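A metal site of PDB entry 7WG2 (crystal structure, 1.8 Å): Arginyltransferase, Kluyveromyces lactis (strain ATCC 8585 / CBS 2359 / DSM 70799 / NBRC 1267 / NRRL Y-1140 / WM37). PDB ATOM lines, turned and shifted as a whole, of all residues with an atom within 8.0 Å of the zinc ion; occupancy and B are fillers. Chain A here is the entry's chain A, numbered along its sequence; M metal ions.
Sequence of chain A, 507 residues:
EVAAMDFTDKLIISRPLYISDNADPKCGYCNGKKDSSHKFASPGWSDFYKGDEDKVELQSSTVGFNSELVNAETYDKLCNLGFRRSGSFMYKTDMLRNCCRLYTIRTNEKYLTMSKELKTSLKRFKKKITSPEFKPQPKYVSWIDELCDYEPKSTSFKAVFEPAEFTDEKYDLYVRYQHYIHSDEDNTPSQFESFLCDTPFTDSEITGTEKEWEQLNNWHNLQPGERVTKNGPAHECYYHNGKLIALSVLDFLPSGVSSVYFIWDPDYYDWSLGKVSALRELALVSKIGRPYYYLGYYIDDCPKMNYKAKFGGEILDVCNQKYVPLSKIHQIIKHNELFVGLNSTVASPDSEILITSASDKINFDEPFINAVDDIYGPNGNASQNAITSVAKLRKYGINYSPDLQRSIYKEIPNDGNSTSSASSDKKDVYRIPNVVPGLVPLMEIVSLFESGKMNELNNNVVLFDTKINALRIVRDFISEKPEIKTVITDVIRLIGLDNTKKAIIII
ND2 of Asn 336 lies within hydrogen-bond range of O of Cys 99.
ND2 of Asn 98 is in hydrogen-bond range of O of Cys 100 (2.8 Å).
The backbone NH (N) of Gly 32 lies close to the side-chain sulfur (SG) of Cys 30 (3.2 Å).
The backbone NH (N) of Cys 99 lies within hydrogen-bond range of the backbone carbonyl oxygen (O) of Gln 59 (2.9 Å).
SG of Cys 100 sits close to NZ of Lys 34 (3.3 Å).
The backbone carbonyl oxygen (O) of Cys 27 sits close to the side-chain amide nitrogen (ND2) of Asn 31, 3.5 Å away.
SG of Cys 27 lies close to N of Tyr 29.
Four residues have an atom within 4 Å of the zinc ion: Cys 27, Cys 30, Cys 99 and Cys 100.
The zinc ion is bound by SG of Cys 30 (2.3 Å), SG of Cys 100 (2.3 Å), SG of Cys 99 (2.3 Å) and SG of Cys 27 (2.4 Å).
The zinc ion has four donor atoms within binding distance.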
ATOM      1  N   ALA A  23     -29.697  25.395  10.642  1.00  0.00           N
ATOM      2  CA  ALA A  23     -29.118  24.448  11.579  1.00  0.00           C
ATOM      3  C   ALA A  23     -29.579  24.726  13.008  1.00  0.00           C
ATOM      4  O   ALA A  23     -29.637  23.816  13.828  1.00  0.00           O
ATOM      5  CB  ALA A  23     -27.584  24.513  11.509  1.00  0.00           C
ATOM      6  N   ASP A  24     -29.822  25.992  13.327  1.00  0.00           N
ATOM      7  CA  ASP A  24     -30.515  26.345  14.552  1.00  0.00           C
ATOM      8  C   ASP A  24     -31.994  26.382  14.214  1.00  0.00           C
ATOM      9  O   ASP A  24     -32.444  27.344  13.562  1.00  0.00           O
ATOM     10  CB  ASP A  24     -30.040  27.686  15.060  1.00  0.00           C
ATOM     11  CG  ASP A  24     -30.763  28.116  16.320  1.00  0.00           C
ATOM     12  OD1 ASP A  24     -31.722  27.429  16.742  1.00  0.00           O
ATOM     13  OD2 ASP A  24     -30.359  29.148  16.874  1.00  0.00           O
ATOM     14  N   LYS A  26     -32.468  22.788  13.580  1.00  0.00           N
ATOM     15  CA  LYS A  26     -32.548  21.469  12.934  1.00  0.00           C
ATOM     16  C   LYS A  26     -31.401  20.544  13.317  1.00  0.00           C
ATOM     17  O   LYS A  26     -31.594  19.324  13.391  1.00  0.00           O
ATOM     18  CB  LYS A  26     -32.576  21.628  11.426  1.00  0.00           C
ATOM     19  CG  LYS A  26     -32.735  20.319  10.665  1.00  0.00           C
ATOM     20  CD  LYS A  26     -32.808  20.581   9.178  1.00  0.00           C
ATOM     21  CE  LYS A  26     -32.531  19.304   8.398  1.00  0.00           C
ATOM     22  NZ  LYS A  26     -32.796  19.473   6.972  1.00  0.00           N
ATOM     23  N   CYS A  27     -30.177  21.067  13.469  1.00  0.00           N
ATOM     24  CA  CYS A  27     -29.029  20.198  13.739  1.00  0.00           C
ATOM     25  C   CYS A  27     -28.958  19.872  15.228  1.00  0.00           C
ATOM     26  O   CYS A  27     -28.703  20.764  16.043  1.00  0.00           O
ATOM     27  CB  CYS A  27     -27.692  20.828  13.310  1.00  0.00           C
ATOM     28  SG  CYS A  27     -26.389  19.628  13.572  1.00  0.00           S
ATOM     29  N   GLY A  28     -29.129  18.605  15.580  1.00  0.00           N
ATOM     30  CA  GLY A  28     -29.022  18.219  16.955  1.00  0.00           C
ATOM     31  C   GLY A  28     -27.597  18.008  17.430  1.00  0.00           C
ATOM     32  O   GLY A  28     -27.373  17.790  18.617  1.00  0.00           O
ATOM     33  N   TYR A  29     -26.616  18.106  16.527  1.00  0.00           N
ATOM     34  CA  TYR A  29     -25.225  17.997  16.953  1.00  0.00           C
ATOM     35  C   TYR A  29     -24.667  19.320  17.445  1.00  0.00           C
ATOM     36  O   TYR A  29     -23.984  19.348  18.471  1.00  0.00           O
ATOM     37  CB  TYR A  29     -24.365  17.459  15.830  1.00  0.00           C
ATOM     38  CG  TYR A  29     -24.887  16.190  15.211  1.00  0.00           C
ATOM     39  CD1 TYR A  29     -25.030  15.042  15.961  1.00  0.00           C
ATOM     40  CD2 TYR A  29     -25.226  16.145  13.858  1.00  0.00           C
ATOM     41  CE1 TYR A  29     -25.523  13.867  15.376  1.00  0.00           C
ATOM     42  CE2 TYR A  29     -25.710  15.005  13.283  1.00  0.00           C
ATOM     43  CZ  TYR A  29     -25.828  13.874  14.037  1.00  0.00           C
ATOM     44  OH  TYR A  29     -26.308  12.743  13.422  1.00  0.00           O
ATOM     45  N   CYS A  30     -24.925  20.416  16.731  1.00  0.00           N
ATOM     46  CA  CYS A  30     -24.341  21.723  17.024  1.00  0.00           C
ATOM     47  C   CYS A  30     -25.394  22.783  17.314  1.00  0.00           C
ATOM     48  O   CYS A  30     -25.048  23.867  17.796  1.00  0.00           O
ATOM     49  CB  CYS A  30     -23.472  22.197  15.851  1.00  0.00           C
ATOM     50  SG  CYS A  30     -24.375  22.834  14.359  1.00  0.00           S
ATOM     51  N   ASN A  31     -26.668  22.507  17.016  1.00  0.00           N
ATOM     52  CA  ASN A  31     -27.745  23.463  17.253  1.00  0.00           C
ATOM     53  C   ASN A  31     -27.478  24.785  16.530  1.00  0.00           C
ATOM     54  O   ASN A  31     -28.008  25.847  16.917  1.00  0.00           O
ATOM     55  CB  ASN A  31     -27.981  23.696  18.750  1.00  0.00           C
ATOM     56  CG  ASN A  31     -27.823  22.411  19.584  1.00  0.00           C
ATOM     57  OD1 ASN A  31     -26.848  22.236  20.358  1.00  0.00           O
ATOM     58  ND2 ASN A  31     -28.753  21.515  19.427  1.00  0.00           N
ATOM     59  N   GLY A  32     -26.711  24.736  15.463  1.00  0.00           N
ATOM     60  CA  GLY A  32     -26.391  25.904  14.701  1.00  0.00           C
ATOM     61  C   GLY A  32     -25.334  26.796  15.325  1.00  0.00           C
ATOM     62  O   GLY A  32     -25.148  27.912  14.837  1.00  0.00           O
ATOM     63  N   LYS A  33     -24.636  26.318  16.354  1.00  0.00           N
ATOM     64  CA  LYS A  33     -23.689  27.147  17.123  1.00  0.00           C
ATOM     65  C   LYS A  33     -22.264  26.707  16.843  1.00  0.00           C
ATOM     66  O   LYS A  33     -21.833  25.655  17.321  1.00  0.00           O
ATOM     67  CB  LYS A  33     -23.952  27.049  18.623  1.00  0.00           C
ATOM     68  CG  LYS A  33     -25.338  27.386  19.054  1.00  0.00           C
ATOM     69  CD  LYS A  33     -25.801  28.690  18.433  1.00  0.00           C
ATOM     70  CE  LYS A  33     -27.215  29.086  18.930  1.00  0.00           C
ATOM     71  NZ  LYS A  33     -27.942  27.938  19.562  1.00  0.00           N
ATOM     72  N   LYS A  34     -21.518  27.553  16.138  1.00  0.00           N
ATOM     73  CA  LYS A  34     -20.115  27.303  15.830  1.00  0.00           C
ATOM     74  C   LYS A  34     -19.286  28.558  16.013  1.00  0.00           C
ATOM     75  O   LYS A  34     -19.737  29.672  15.743  1.00  0.00           O
ATOM     76  CB  LYS A  34     -19.946  26.814  14.377  1.00  0.00           C
ATOM     77  CG  LYS A  34     -20.685  25.526  14.098  1.00  0.00           C
ATOM     78  CD  LYS A  34     -19.747  24.346  14.218  1.00  0.00           C
ATOM     79  CE  LYS A  34     -20.408  23.087  13.727  1.00  0.00           C
ATOM     80  NZ  LYS A  34     -20.165  21.968  14.643  1.00  0.00           N
ATOM     81  N   LEU A  58     -25.937  29.139   9.154  1.00  0.00           N
ATOM     82  CA  LEU A  58     -25.636  27.739   8.918  1.00  0.00           C
ATOM     83  C   LEU A  58     -26.905  26.944   8.642  1.00  0.00           C
ATOM     84  O   LEU A  58     -27.926  27.142   9.299  1.00  0.00           O
ATOM     85  CB  LEU A  58     -24.929  27.162  10.143  1.00  0.00           C
ATOM     86  CG  LEU A  58     -23.457  27.600  10.288  1.00  0.00           C
ATOM     87  CD1 LEU A  58     -22.862  26.884  11.477  1.00  0.00           C
ATOM     88  CD2 LEU A  58     -22.668  27.285   9.057  1.00  0.00           C
ATOM     89  N   GLN A  59     -26.836  26.051   7.648  1.00  0.00           N
ATOM     90  CA  GLN A  59     -27.923  25.157   7.282  1.00  0.00           C
ATOM     91  C   GLN A  59     -27.558  23.722   7.636  1.00  0.00           C
ATOM     92  O   GLN A  59     -26.372  23.371   7.688  1.00  0.00           O
ATOM     93  CB  GLN A  59     -28.206  25.243   5.783  1.00  0.00           C
ATOM     94  CG  GLN A  59     -28.487  26.641   5.302  1.00  0.00           C
ATOM     95  CD  GLN A  59     -29.755  27.210   5.880  1.00  0.00           C
ATOM     96  OE1 GLN A  59     -30.849  26.776   5.545  1.00  0.00           O
ATOM     97  NE2 GLN A  59     -29.626  28.215   6.743  1.00  0.00           N
ATOM     98  N   SER A  60     -28.572  22.913   7.899  1.00  0.00           N
ATOM     99  CA  SER A  60     -28.418  21.477   8.056  1.00  0.00           C
ATOM    100  C   SER A  60     -29.183  20.841   6.907  1.00  0.00           C
ATOM    101  O   SER A  60     -30.334  21.170   6.678  1.00  0.00           O
ATOM    102  CB  SER A  60     -28.948  21.009   9.407  1.00  0.00           C
ATOM    103  OG  SER A  60     -28.809  19.607   9.529  1.00  0.00           O
ATOM    104  N   SER A  61     -28.516  19.971   6.164  1.00  0.00           N
ATOM    105  CA  SER A  61     -29.084  19.511   4.902  1.00  0.00           C
ATOM    106  C   SER A  61     -28.731  18.061   4.636  1.00  0.00           C
ATOM    107  O   SER A  61     -27.555  17.670   4.759  1.00  0.00           O
ATOM    108  CB  SER A  61     -28.545  20.362   3.768  1.00  0.00           C
ATOM    109  OG  SER A  61     -27.175  20.039   3.607  1.00  0.00           O
ATOM    110  N   ASN A  98     -23.443  21.384   4.820  1.00  0.00           N
ATOM    111  CA  ASN A  98     -23.927  21.116   6.165  1.00  0.00           C
ATOM    112  C   ASN A  98     -23.104  21.847   7.240  1.00  0.00           C
ATOM    113  O   ASN A  98     -21.880  22.058   7.115  1.00  0.00           O
ATOM    114  CB  ASN A  98     -23.899  19.610   6.454  1.00  0.00           C
ATOM    115  CG  ASN A  98     -24.847  19.214   7.571  1.00  0.00           C
ATOM    116  OD1 ASN A  98     -26.042  19.467   7.499  1.00  0.00           O
ATOM    117  ND2 ASN A  98     -24.328  18.590   8.603  1.00  0.00           N
ATOM    118  N   CYS A  99     -23.797  22.200   8.324  1.00  0.00           N
ATOM    119  CA  CYS A  99     -23.143  22.865   9.454  1.00  0.00           C
ATOM    120  C   CYS A  99     -22.004  22.013  10.016  1.00  0.00           C
ATOM    121  O   CYS A  99     -20.917  22.526  10.308  1.00  0.00           O
ATOM    122  CB  CYS A  99     -24.202  23.142  10.529  1.00  0.00           C
ATOM    123  SG  CYS A  99     -25.266  21.688  10.868  1.00  0.00           S
ATOM    124  N   CYS A 100     -22.249  20.720  10.153  1.00  0.00           N
ATOM    125  CA  CYS A 100     -21.329  19.766  10.752  1.00  0.00           C
ATOM    126  C   CYS A 100     -20.791  18.826   9.695  1.00  0.00           C
ATOM    127  O   CYS A 100     -21.521  18.364   8.792  1.00  0.00           O
ATOM    128  CB  CYS A 100     -22.037  18.946  11.837  1.00  0.00           C
ATOM    129  SG  CYS A 100     -22.454  19.919  13.330  1.00  0.00           S
ATOM    130  N   ARG A 101     -19.515  18.486   9.823  1.00  0.00           N
ATOM    131  CA  ARG A 101     -18.870  17.535   8.906  1.00  0.00           C
ATOM    132  C   ARG A 101     -19.012  16.124   9.479  1.00  0.00           C
ATOM    133  O   ARG A 101     -18.386  15.782  10.502  1.00  0.00           O
ATOM    134  CB  ARG A 101     -17.405  17.882   8.676  1.00  0.00           C
ATOM    135  CG  ARG A 101     -16.961  17.648   7.203  1.00  0.00           C
ATOM    136  CD  ARG A 101     -17.639  18.613   6.189  1.00  0.00           C
ATOM    137  NE  ARG A 101     -17.392  19.997   6.597  1.00  0.00           N
ATOM    138  CZ  ARG A 101     -18.346  20.909   6.744  1.00  0.00           C
ATOM    139  NH1 ARG A 101     -19.553  20.751   6.201  1.00  0.00           N
ATOM    140  NH2 ARG A 101     -18.103  21.981   7.493  1.00  0.00           N
ATOM    141  N   LEU A 102     -19.810  15.304   8.815  1.00  0.00           N
ATOM    142  CA  LEU A 102     -20.075  13.930   9.225  1.00  0.00           C
ATOM    143  C   LEU A 102     -19.278  12.993   8.322  1.00  0.00           C
ATOM    144  O   LEU A 102     -19.369  13.070   7.099  1.00  0.00           O
ATOM    145  CB  LEU A 102     -21.571  13.624   9.114  1.00  0.00           C
ATOM    146  CG  LEU A 102     -22.398  14.041  10.326  1.00  0.00           C
ATOM    147  CD1 LEU A 102     -22.484  15.536  10.423  1.00  0.00           C
ATOM    148  CD2 LEU A 102     -23.803  13.469  10.215  1.00  0.00           C
ATOM    149  N   ILE A 299     -18.106  12.889  13.995  1.00  0.00           N
ATOM    150  CA  ILE A 299     -17.985  14.345  13.864  1.00  0.00           C
ATOM    151  C   ILE A 299     -16.897  14.779  14.827  1.00  0.00           C
ATOM    152  O   ILE A 299     -17.064  14.616  16.040  1.00  0.00           O
ATOM    153  CB  ILE A 299     -19.294  15.073  14.199  1.00  0.00           C
ATOM    154  CG1 ILE A 299     -20.500  14.563  13.390  1.00  0.00           C
ATOM    155  CG2 ILE A 299     -19.137  16.551  13.931  1.00  0.00           C
ATOM    156  CD1 ILE A 299     -21.873  15.115  13.859  1.00  0.00           C
ATOM    157  N   ASP A 301     -15.757  17.564  16.055  1.00  0.00           N
ATOM    158  CA  ASP A 301     -16.003  18.566  17.089  1.00  0.00           C
ATOM    159  C   ASP A 301     -17.270  18.296  17.918  1.00  0.00           C
ATOM    160  O   ASP A 301     -17.712  19.199  18.647  1.00  0.00           O
ATOM    161  CB  ASP A 301     -16.043  19.973  16.475  1.00  0.00           C
ATOM    162  CG  ASP A 301     -17.319  20.265  15.648  1.00  0.00           C
ATOM    163  OD1 ASP A 301     -18.181  19.370  15.523  1.00  0.00           O
ATOM    164  OD2 ASP A 301     -17.429  21.407  15.110  1.00  0.00           O
ATOM    165  N   CYS A 302     -17.826  17.078  17.880  1.00  0.00           N
ATOM    166  CA  CYS A 302     -19.004  16.707  18.675  1.00  0.00           C
ATOM    167  C   CYS A 302     -18.733  15.569  19.646  1.00  0.00           C
ATOM    168  O   CYS A 302     -18.580  14.415  19.218  1.00  0.00           O
ATOM    169  CB  CYS A 302     -20.145  16.300  17.723  1.00  0.00           C
ATOM    170  SG  CYS A 302     -21.697  16.013  18.585  1.00  0.00           S
ATOM    171  N   ASN A 336     -13.494  21.054  11.727  1.00  0.00           N
ATOM    172  CA  ASN A 336     -14.753  20.797  11.036  1.00  0.00           C
ATOM    173  C   ASN A 336     -14.624  20.929   9.523  1.00  0.00           C
ATOM    174  O   ASN A 336     -15.630  21.131   8.824  1.00  0.00           O
ATOM    175  CB  ASN A 336     -15.844  21.739  11.585  1.00  0.00           C
ATOM    176  CG  ASN A 336     -17.264  21.263  11.257  1.00  0.00           C
ATOM    177  OD1 ASN A 336     -17.610  20.074  11.365  1.00  0.00           O
ATOM    178  ND2 ASN A 336     -18.087  22.197  10.877  1.00  0.00           N
HETATM  179 ZN    ZN M   1     -24.506  20.989  12.976  1.00  0.00          ZN
